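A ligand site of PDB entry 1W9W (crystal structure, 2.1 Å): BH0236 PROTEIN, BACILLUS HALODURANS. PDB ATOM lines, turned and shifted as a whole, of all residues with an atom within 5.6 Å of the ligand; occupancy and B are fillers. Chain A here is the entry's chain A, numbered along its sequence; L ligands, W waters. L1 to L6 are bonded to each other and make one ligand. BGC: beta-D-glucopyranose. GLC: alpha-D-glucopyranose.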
ATOM      1  N   GLU A  29     -10.623  10.446 -29.174  1.00  0.00           N
ATOM      2  CA  GLU A  29     -10.032  10.268 -30.526  1.00  0.00           C
ATOM      3  C   GLU A  29     -11.124  10.659 -31.526  1.00  0.00           C
ATOM      4  O   GLU A  29     -12.316  10.684 -31.175  1.00  0.00           O
ATOM      5  CB  GLU A  29      -9.643   8.783 -30.771  1.00  0.00           C
ATOM      6  CG  GLU A  29     -10.884   7.859 -30.823  1.00  0.00           C
ATOM      7  CD  GLU A  29     -10.569   6.346 -30.815  1.00  0.00           C
ATOM      8  OE1 GLU A  29      -9.522   5.958 -31.326  1.00  0.00           O
ATOM      9  OE2 GLU A  29     -11.381   5.529 -30.301  1.00  0.00           O
ATOM     10  N   ASN A  39     -15.042  10.211 -30.281  1.00  0.00           N
ATOM     11  CA  ASN A  39     -15.622   9.284 -29.291  1.00  0.00           C
ATOM     12  C   ASN A  39     -14.690   9.308 -28.091  1.00  0.00           C
ATOM     13  O   ASN A  39     -13.541   9.784 -28.198  1.00  0.00           O
ATOM     14  CB  ASN A  39     -15.787   7.855 -29.838  1.00  0.00           C
ATOM     15  CG  ASN A  39     -14.486   7.284 -30.372  1.00  0.00           C
ATOM     16  OD1 ASN A  39     -14.168   7.452 -31.561  1.00  0.00           O
ATOM     17  ND2 ASN A  39     -13.677   6.668 -29.482  1.00  0.00           N
ATOM     18  N   ILE A  40     -15.180   8.868 -26.941  1.00  0.00           N
ATOM     19  CA  ILE A  40     -14.289   8.557 -25.806  1.00  0.00           C
ATOM     20  C   ILE A  40     -13.891   7.087 -25.950  1.00  0.00           C
ATOM     21  O   ILE A  40     -14.529   6.318 -26.671  1.00  0.00           O
ATOM     22  CB  ILE A  40     -14.929   8.901 -24.456  1.00  0.00           C
ATOM     23  CG1 ILE A  40     -16.201   8.075 -24.239  1.00  0.00           C
ATOM     24  CG2 ILE A  40     -15.247  10.418 -24.378  1.00  0.00           C
ATOM     25  CD1 ILE A  40     -16.852   8.242 -22.890  1.00  0.00           C
ATOM     26  N   GLY A  41     -12.792   6.726 -25.314  1.00  0.00           N
ATOM     27  CA  GLY A  41     -12.211   5.417 -25.465  1.00  0.00           C
ATOM     28  C   GLY A  41     -11.217   5.186 -24.379  1.00  0.00           C
ATOM     29  O   GLY A  41     -10.991   6.033 -23.489  1.00  0.00           O
ATOM     30  N   TRP A  42     -10.504   4.065 -24.488  1.00  0.00           N
ATOM     31  CA  TRP A  42      -9.555   3.691 -23.447  1.00  0.00           C
ATOM     32  C   TRP A  42     -10.285   3.574 -22.103  1.00  0.00           C
ATOM     33  O   TRP A  42      -9.786   3.984 -21.041  1.00  0.00           O
ATOM     34  CB  TRP A  42      -8.380   4.653 -23.388  1.00  0.00           C
ATOM     35  CG  TRP A  42      -7.500   4.531 -24.553  1.00  0.00           C
ATOM     36  CD1 TRP A  42      -6.414   3.728 -24.665  1.00  0.00           C
ATOM     37  CD2 TRP A  42      -7.625   5.212 -25.806  1.00  0.00           C
ATOM     38  NE1 TRP A  42      -5.859   3.852 -25.913  1.00  0.00           N
ATOM     39  CE2 TRP A  42      -6.564   4.773 -26.626  1.00  0.00           C
ATOM     40  CE3 TRP A  42      -8.525   6.146 -26.313  1.00  0.00           C
ATOM     41  CZ2 TRP A  42      -6.374   5.242 -27.932  1.00  0.00           C
ATOM     42  CZ3 TRP A  42      -8.346   6.619 -27.607  1.00  0.00           C
ATOM     43  CH2 TRP A  42      -7.278   6.162 -28.413  1.00  0.00           C
ATOM     44  N   ILE A  43     -11.486   2.991 -22.166  1.00  0.00           N
ATOM     45  CA  ILE A  43     -12.350   2.867 -21.000  1.00  0.00           C
ATOM     46  C   ILE A  43     -12.059   1.531 -20.298  1.00  0.00           C
ATOM     47  O   ILE A  43     -11.995   0.537 -20.963  1.00  0.00           O
ATOM     48  CB  ILE A  43     -13.807   2.912 -21.455  1.00  0.00           C
ATOM     49  CG1 ILE A  43     -14.157   4.361 -21.927  1.00  0.00           C
ATOM     50  CG2 ILE A  43     -14.768   2.356 -20.345  1.00  0.00           C
ATOM     51  CD1 ILE A  43     -15.513   4.483 -22.783  1.00  0.00           C
ATOM     52  N   ASP A  70     -14.228  -4.004 -29.176  1.00  0.00           N
ATOM     53  CA  ASP A  70     -13.449  -5.083 -29.785  1.00  0.00           C
ATOM     54  C   ASP A  70     -13.162  -6.178 -28.755  1.00  0.00           C
ATOM     55  O   ASP A  70     -12.416  -7.130 -29.028  1.00  0.00           O
ATOM     56  CB  ASP A  70     -12.185  -4.517 -30.440  1.00  0.00           C
ATOM     57  CG  ASP A  70     -11.462  -5.530 -31.289  1.00  0.00           C
ATOM     58  OD1 ASP A  70     -12.189  -6.302 -31.944  1.00  0.00           O
ATOM     59  OD2 ASP A  70     -10.193  -5.614 -31.375  1.00  0.00           O
ATOM     60  N   THR A  71     -13.791  -6.085 -27.593  1.00  0.00           N
ATOM     61  CA  THR A  71     -13.553  -7.010 -26.502  1.00  0.00           C
ATOM     62  C   THR A  71     -14.884  -7.648 -26.077  1.00  0.00           C
ATOM     63  O   THR A  71     -15.884  -7.438 -26.695  1.00  0.00           O
ATOM     64  CB  THR A  71     -12.796  -6.265 -25.344  1.00  0.00           C
ATOM     65  OG1 THR A  71     -13.605  -5.201 -24.766  1.00  0.00           O
ATOM     66  CG2 THR A  71     -11.499  -5.587 -25.889  1.00  0.00           C
ATOM     67  N   PRO A  72     -14.908  -8.480 -25.042  1.00  0.00           N
ATOM     68  CA  PRO A  72     -16.194  -8.931 -24.500  1.00  0.00           C
ATOM     69  C   PRO A  72     -17.137  -7.817 -24.062  1.00  0.00           C
ATOM     70  O   PRO A  72     -18.327  -8.081 -23.951  1.00  0.00           O
ATOM     71  CB  PRO A  72     -15.799  -9.799 -23.327  1.00  0.00           C
ATOM     72  CG  PRO A  72     -14.357 -10.293 -23.693  1.00  0.00           C
ATOM     73  CD  PRO A  72     -13.770  -9.060 -24.311  1.00  0.00           C
ATOM     74  N   ASN A  95     -19.582  -7.038 -27.524  1.00  0.00           N
ATOM     75  CA  ASN A  95     -18.700  -6.973 -28.635  1.00  0.00           C
ATOM     76  C   ASN A  95     -19.540  -6.597 -29.812  1.00  0.00           C
ATOM     77  O   ASN A  95     -20.672  -7.061 -29.905  1.00  0.00           O
ATOM     78  CB  ASN A  95     -18.019  -8.286 -28.896  1.00  0.00           C
ATOM     79  CG  ASN A  95     -16.996  -8.167 -29.962  1.00  0.00           C
ATOM     80  OD1 ASN A  95     -15.858  -7.750 -29.707  1.00  0.00           O
ATOM     81  ND2 ASN A  95     -17.381  -8.444 -31.166  1.00  0.00           N
ATOM     82  N   THR A  96     -18.984  -5.785 -30.699  1.00  0.00           N
ATOM     83  CA  THR A  96     -19.651  -5.295 -31.867  1.00  0.00           C
ATOM     84  C   THR A  96     -18.801  -5.484 -33.090  1.00  0.00           C
ATOM     85  O   THR A  96     -19.220  -5.026 -34.131  1.00  0.00           O
ATOM     86  CB  THR A  96     -19.906  -3.740 -31.795  1.00  0.00           C
ATOM     87  OG1 THR A  96     -18.648  -3.025 -31.795  1.00  0.00           O
ATOM     88  CG2 THR A  96     -20.658  -3.340 -30.560  1.00  0.00           C
ATOM     89  N   GLY A  97     -17.617  -6.088 -32.985  1.00  0.00           N
ATOM     90  CA  GLY A  97     -16.834  -6.368 -34.186  1.00  0.00           C
ATOM     91  C   GLY A  97     -15.595  -5.540 -34.353  1.00  0.00           C
ATOM     92  O   GLY A  97     -14.773  -5.829 -35.230  1.00  0.00           O
ATOM     93  N   GLY A  98     -15.445  -4.514 -33.527  1.00  0.00           N
ATOM     94  CA  GLY A  98     -14.396  -3.518 -33.703  1.00  0.00           C
ATOM     95  C   GLY A  98     -14.568  -2.262 -32.839  1.00  0.00           C
ATOM     96  O   GLY A  98     -15.675  -1.962 -32.342  1.00  0.00           O
ATOM     97  N   TRP A  99     -13.437  -1.594 -32.611  1.00  0.00           N
ATOM     98  CA  TRP A  99     -13.370  -0.297 -31.916  1.00  0.00           C
ATOM     99  C   TRP A  99     -14.139   0.803 -32.642  1.00  0.00           C
ATOM    100  O   TRP A  99     -14.627   1.761 -31.987  1.00  0.00           O
ATOM    101  CB  TRP A  99     -11.910   0.152 -31.784  1.00  0.00           C
ATOM    102  CG  TRP A  99     -11.174  -0.672 -30.817  1.00  0.00           C
ATOM    103  CD1 TRP A  99      -9.988  -1.338 -31.037  1.00  0.00           C
ATOM    104  CD2 TRP A  99     -11.603  -1.011 -29.487  1.00  0.00           C
ATOM    105  NE1 TRP A  99      -9.652  -2.050 -29.904  1.00  0.00           N
ATOM    106  CE2 TRP A  99     -10.613  -1.842 -28.936  1.00  0.00           C
ATOM    107  CE3 TRP A  99     -12.701  -0.643 -28.691  1.00  0.00           C
ATOM    108  CZ2 TRP A  99     -10.683  -2.326 -27.603  1.00  0.00           C
ATOM    109  CZ3 TRP A  99     -12.786  -1.117 -27.399  1.00  0.00           C
ATOM    110  CH2 TRP A  99     -11.781  -1.963 -26.869  1.00  0.00           C
ATOM    111  N   GLN A 100     -14.222   0.674 -33.965  1.00  0.00           N
ATOM    112  CA  GLN A 100     -14.978   1.610 -34.788  1.00  0.00           C
ATOM    113  C   GLN A 100     -16.140   0.967 -35.551  1.00  0.00           C
ATOM    114  O   GLN A 100     -16.473   1.385 -36.676  1.00  0.00           O
ATOM    115  CB  GLN A 100     -14.040   2.366 -35.735  1.00  0.00           C
ATOM    116  CG  GLN A 100     -13.091   3.302 -34.969  1.00  0.00           C
ATOM    117  CD  GLN A 100     -13.798   4.476 -34.224  1.00  0.00           C
ATOM    118  OE1 GLN A 100     -14.965   4.832 -34.530  1.00  0.00           O
ATOM    119  NE2 GLN A 100     -13.094   5.059 -33.242  1.00  0.00           N
ATOM    120  N   TYR A 128      -9.239  -6.096 -19.791  1.00  0.00           N
ATOM    121  CA  TYR A 128      -9.189  -5.484 -21.102  1.00  0.00           C
ATOM    122  C   TYR A 128     -10.012  -4.179 -21.124  1.00  0.00           C
ATOM    123  O   TYR A 128     -10.882  -3.943 -20.262  1.00  0.00           O
ATOM    124  CB  TYR A 128      -9.663  -6.468 -22.168  1.00  0.00           C
ATOM    125  CG  TYR A 128     -10.888  -7.225 -21.715  1.00  0.00           C
ATOM    126  CD1 TYR A 128     -12.129  -6.617 -21.678  1.00  0.00           C
ATOM    127  CD2 TYR A 128     -10.801  -8.541 -21.266  1.00  0.00           C
ATOM    128  CE1 TYR A 128     -13.253  -7.294 -21.252  1.00  0.00           C
ATOM    129  CE2 TYR A 128     -11.926  -9.242 -20.823  1.00  0.00           C
ATOM    130  CZ  TYR A 128     -13.147  -8.609 -20.819  1.00  0.00           C
ATOM    131  OH  TYR A 128     -14.294  -9.261 -20.341  1.00  0.00           O
ATOM    132  N   ASP A 129      -9.744  -3.339 -22.116  1.00  0.00           N
ATOM    133  CA  ASP A 129     -10.520  -2.139 -22.324  1.00  0.00           C
ATOM    134  C   ASP A 129     -11.956  -2.602 -22.714  1.00  0.00           C
ATOM    135  O   ASP A 129     -12.144  -3.701 -23.253  1.00  0.00           O
ATOM    136  CB  ASP A 129      -9.886  -1.214 -23.402  1.00  0.00           C
ATOM    137  CG  ASP A 129      -8.418  -0.807 -23.068  1.00  0.00           C
ATOM    138  OD1 ASP A 129      -8.002  -0.724 -21.859  1.00  0.00           O
ATOM    139  OD2 ASP A 129      -7.591  -0.578 -23.997  1.00  0.00           O
ATOM    140  N   MET A 131     -14.842  -0.646 -24.183  1.00  0.00           N
ATOM    141  CA  MET A 131     -15.712  -0.010 -25.169  1.00  0.00           C
ATOM    142  C   MET A 131     -15.284   1.412 -25.501  1.00  0.00           C
ATOM    143  O   MET A 131     -14.519   2.040 -24.772  1.00  0.00           O
ATOM    144  CB  MET A 131     -17.147   0.089 -24.638  1.00  0.00           C
ATOM    145  CG  MET A 131     -17.299   1.013 -23.449  1.00  0.00           C
ATOM    146  SD  MET A 131     -18.901   1.133 -22.721  1.00  0.00           S
ATOM    147  CE  MET A 131     -18.747  -0.054 -21.299  1.00  0.00           C
ATOM    148  N   ASN A 132     -15.843   1.867 -26.611  1.00  0.00           N
ATOM    149  CA  ASN A 132     -15.926   3.241 -27.013  1.00  0.00           C
ATOM    150  C   ASN A 132     -17.351   3.720 -27.032  1.00  0.00           C
ATOM    151  O   ASN A 132     -18.340   2.984 -27.298  1.00  0.00           O
ATOM    152  CB  ASN A 132     -15.343   3.414 -28.432  1.00  0.00           C
ATOM    153  CG  ASN A 132     -13.904   3.175 -28.474  1.00  0.00           C
ATOM    154  OD1 ASN A 132     -13.246   3.221 -27.445  1.00  0.00           O
ATOM    155  ND2 ASN A 132     -13.353   2.950 -29.675  1.00  0.00           N
HETATM  156  C2  BGC L   1     -14.863 -10.601 -34.321  1.00  0.00           C
HETATM  157  C3  BGC L   1     -13.521 -10.705 -33.606  1.00  0.00           C
HETATM  158  C4  BGC L   1     -12.827 -11.968 -34.184  1.00  0.00           C
HETATM  159  C5  BGC L   1     -12.637 -11.788 -35.707  1.00  0.00           C
HETATM  160  C6  BGC L   1     -12.319 -13.133 -36.412  1.00  0.00           C
HETATM  161  C1  BGC L   1     -14.470 -10.142 -35.729  1.00  0.00           C
HETATM  162  O1  BGC L   1     -15.543  -9.683 -36.549  1.00  0.00           O
HETATM  163  O2  BGC L   1     -15.713  -9.741 -33.620  1.00  0.00           O
HETATM  164  O3  BGC L   1     -13.610 -10.325 -32.235  1.00  0.00           O
HETATM  165  O4  BGC L   1     -11.628 -12.402 -33.542  1.00  0.00           O
HETATM  166  O5  BGC L   1     -13.801 -11.245 -36.325  1.00  0.00           O
HETATM  167  O6  BGC L   1     -11.419 -13.107 -37.549  1.00  0.00           O
HETATM  168  C2  BGC L   2     -12.814 -10.463 -30.023  1.00  0.00           C
HETATM  169  C3  BGC L   2     -12.981 -10.927 -28.574  1.00  0.00           C
HETATM  170  C4  BGC L   2     -14.461 -11.109 -28.198  1.00  0.00           C
HETATM  171  C5  BGC L   2     -15.102 -11.878 -29.379  1.00  0.00           C
HETATM  172  C6  BGC L   2     -16.595 -12.155 -29.272  1.00  0.00           C
HETATM  173  C1  BGC L   2     -13.699 -11.135 -31.072  1.00  0.00           C
HETATM  174  O2  BGC L   2     -11.425 -10.579 -30.280  1.00  0.00           O
HETATM  175  O3  BGC L   2     -12.257  -9.904 -27.969  1.00  0.00           O
HETATM  176  O4  BGC L   2     -14.597 -11.784 -26.944  1.00  0.00           O
HETATM  177  O5  BGC L   2     -14.981 -11.077 -30.515  1.00  0.00           O
HETATM  178  O6  BGC L   2     -17.112 -12.892 -30.366  1.00  0.00           O
HETATM  179  C1  GLC L   3     -11.575 -10.015 -26.719  1.00  0.00           C
HETATM  180  C2  GLC L   3     -10.390  -9.010 -26.708  1.00  0.00           C
HETATM  181  C3  GLC L   3      -9.115  -9.510 -26.046  1.00  0.00           C
HETATM  182  C4  GLC L   3      -9.456 -10.352 -24.810  1.00  0.00           C
HETATM  183  C5  GLC L   3     -10.312 -11.547 -25.236  1.00  0.00           C
HETATM  184  C6  GLC L   3     -10.961 -12.351 -24.103  1.00  0.00           C
HETATM  185  O2  GLC L   3     -10.142  -8.386 -27.955  1.00  0.00           O
HETATM  186  O3  GLC L   3      -8.515  -8.336 -25.537  1.00  0.00           O
HETATM  187  O4  GLC L   3      -8.265 -10.694 -24.063  1.00  0.00           O
HETATM  188  O5  GLC L   3     -11.301 -11.295 -26.275  1.00  0.00           O
HETATM  189  O6  GLC L   3     -11.107 -13.728 -24.499  1.00  0.00           O
HETATM  190  C2  BGC L   4      -7.261  -6.348 -26.251  1.00  0.00           C
HETATM  191  C3  BGC L   4      -5.908  -5.912 -26.849  1.00  0.00           C
HETATM  192  C4  BGC L   4      -4.757  -6.739 -26.265  1.00  0.00           C
HETATM  193  C5  BGC L   4      -5.074  -8.258 -26.202  1.00  0.00           C
HETATM  194  C6  BGC L   4      -4.119  -8.928 -25.206  1.00  0.00           C
HETATM  195  C1  BGC L   4      -7.427  -7.872 -26.332  1.00  0.00           C
HETATM  196  O2  BGC L   4      -8.302  -5.631 -26.896  1.00  0.00           O
HETATM  197  O3  BGC L   4      -5.619  -4.607 -26.384  1.00  0.00           O
HETATM  198  O4  BGC L   4      -3.568  -6.512 -27.008  1.00  0.00           O
HETATM  199  O5  BGC L   4      -6.371  -8.596 -25.753  1.00  0.00           O
HETATM  200  O6  BGC L   4      -3.283  -9.556 -26.097  1.00  0.00           O
HETATM  201  C2  BGC L   5      -6.402  -2.309 -26.688  1.00  0.00           C
HETATM  202  C3  BGC L   5      -6.577  -1.229 -27.764  1.00  0.00           C
HETATM  203  C4  BGC L   5      -5.266  -1.103 -28.584  1.00  0.00           C
HETATM  204  C5  BGC L   5      -4.947  -2.498 -29.114  1.00  0.00           C
HETATM  205  C6  BGC L   5      -3.812  -2.570 -30.144  1.00  0.00           C
HETATM  206  C1  BGC L   5      -5.840  -3.595 -27.354  1.00  0.00           C
HETATM  207  O2  BGC L   5      -7.580  -2.579 -25.936  1.00  0.00           O
HETATM  208  O3  BGC L   5      -6.898   0.026 -27.182  1.00  0.00           O
HETATM  209  O4  BGC L   5      -5.405  -0.214 -29.668  1.00  0.00           O
HETATM  210  O5  BGC L   5      -4.630  -3.278 -27.988  1.00  0.00           O
HETATM  211  O6  BGC L   5      -2.650  -2.330 -29.416  1.00  0.00           O
HETATM  212  C2  BGC L   6      -8.818   1.528 -26.970  1.00  0.00           C
HETATM  213  C3  BGC L   6      -9.962   2.107 -27.827  1.00  0.00           C
HETATM  214  C4  BGC L   6      -9.432   2.778 -29.085  1.00  0.00           C
HETATM  215  C5  BGC L   6      -8.403   1.906 -29.827  1.00  0.00           C
HETATM  216  C6  BGC L   6      -7.650   2.735 -30.898  1.00  0.00           C
HETATM  217  C1  BGC L   6      -7.973   0.660 -27.891  1.00  0.00           C
HETATM  218  O2  BGC L   6      -9.350   0.734 -25.944  1.00  0.00           O
HETATM  219  O3  BGC L   6     -10.853   2.971 -27.150  1.00  0.00           O
HETATM  220  O4  BGC L   6     -10.489   3.012 -29.984  1.00  0.00           O
HETATM  221  O5  BGC L   6      -7.433   1.383 -28.930  1.00  0.00           O
HETATM  222  O6  BGC L   6      -6.824   1.875 -31.677  1.00  0.00           O
HETATM  223  O   HOH W   1      -2.472  -3.658 -25.872  1.00  0.00           O
HETATM  224  O   HOH W   2      -8.602  -4.961 -29.301  1.00  0.00           O
HETATM  225  O   HOH W   3     -10.568   3.565 -32.883  1.00  0.00           O
HETATM  226  O   HOH W   4     -11.769   1.192 -24.761  1.00  0.00           O
HETATM  227  O   HOH W   5     -14.477  -7.540 -31.864  1.00  0.00           O
HETATM  228  O   HOH W   6      -6.404  -8.977 -22.950  1.00  0.00           O
HETATM  229  O   HOH W   7      -1.244  -7.230 -24.667  1.00  0.00           O
HETATM  230  O   HOH W   8      -9.040  -8.913 -30.024  1.00  0.00           O
HETATM  231  O   HOH W   9      -4.922   0.333 -24.466  1.00  0.00           O
HETATM  232  O   HOH W  10     -10.577  -8.811 -32.091  1.00  0.00           O
HETATM  233  O   HOH W  11      -6.641 -11.909 -25.823  1.00  0.00           O
HETATM  234  O   HOH W  12     -13.253 -13.936 -26.161  1.00  0.00           O
HETATM  235  O   HOH W  13     -10.031 -12.790 -30.114  1.00  0.00           O
HETATM  236  O   HOH W  14      -7.406  -4.071 -23.661  1.00  0.00           O
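OD1 of Asn 132 sits at hydrogen-bond distance from O3 of BGC L6, at 2.4 Å. The side-chain carboxylate (OE2) of Glu 29 sits at hydrogen-bond distance from an oxygen (O4) of BGC L6, 2.7 Å away. OD2 of Asp 129 is in hydrogen-bond range of O2 of BGC L5 (2.8 Å). O of Asp 70 is in hydrogen-bond range of O2 of GLC L3 (2.8 Å). The backbone NH of Trp 42 lies within hydrogen-bond range of an oxygen (O3) of BGC L6, 2.9 Å away. ND2 of Asn 95 is in hydrogen-bond range of O2 of BGC L1 (3.2 Å).
Water W2 lies within hydrogen-bond range of O2 of BGC L4, OD2 of Asp 70 and NE1 of Trp 99. Water W10 bridges an oxygen (O2) of BGC L2 (2.7 Å) and the side-chain carboxylate (OD1) of Asp 70 (3.0 Å). Water W14 bridges O2 of BGC L5 (2.7 Å) and N of Asp 129 (2.9 Å). Water W4 lies within hydrogen-bond range of an oxygen (O2) of BGC L6 (2.7 Å), the backbone carbonyl oxygen of Met 131 (2.9 Å), the backbone NH of Trp 42 (3.2 Å) and the backbone NH of Ile 43 (3.2 Å). Water W3 lies within hydrogen-bond range of O4 of BGC L6 (3.0 Å), NE2 of Gln 100 (3.0 Å) and OE1 of Glu 29 (3.0 Å). Water W9 bridges the side-chain carboxylate of Asp 129 and an oxygen (O3) of BGC L5.
OE2 of Glu 29 sits at hydrogen-bond distance from ND2 of Asn 132. The backbone carbonyl oxygen (O) of Trp 99 lies within hydrogen-bond range of the side-chain amide nitrogen (ND2) of Asn 132, 2.9 Å away. The side-chain amide oxygen (OD1) of Asn 132 sits close to the backbone carbonyl oxygen (O) of Ile 40, at 3.4 Å. The side-chain carboxylate of Glu 29 sits at hydrogen-bond distance from the side-chain amide nitrogen of Gln 100, 3.4 Å away. The side-chain carboxylate of Glu 29 is in hydrogen-bond range of the side-chain amide nitrogen of Asn 39 (2.7 Å). O of Asp 129 lies within hydrogen-bond range of OG1 of Thr 71. The side-chain amide oxygen of Asn 95 lies close to the backbone carbonyl oxygen of Thr 71. N of Gly 97 lies close to ND2 of Asn 95 (3.0 Å).
Merely in contact with the ligand: Gly 41 (3.3 Å), Thr 71 (3.4 Å), Pro 72 (3.4 Å), Gly 97 (3.6 Å) and Trp 99 (3.5 Å). Hydrophobic or aromatic side chains within 4 Å of the ligand: Trp 42, Pro 72 and Trp 99. Within 4 Å of the ligand: Glu 29, Gly 41, Trp 42, Asp 70, Thr 71, Pro 72, Asn 95, Gly 97, Trp 99, Asp 129 and Asn 132.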
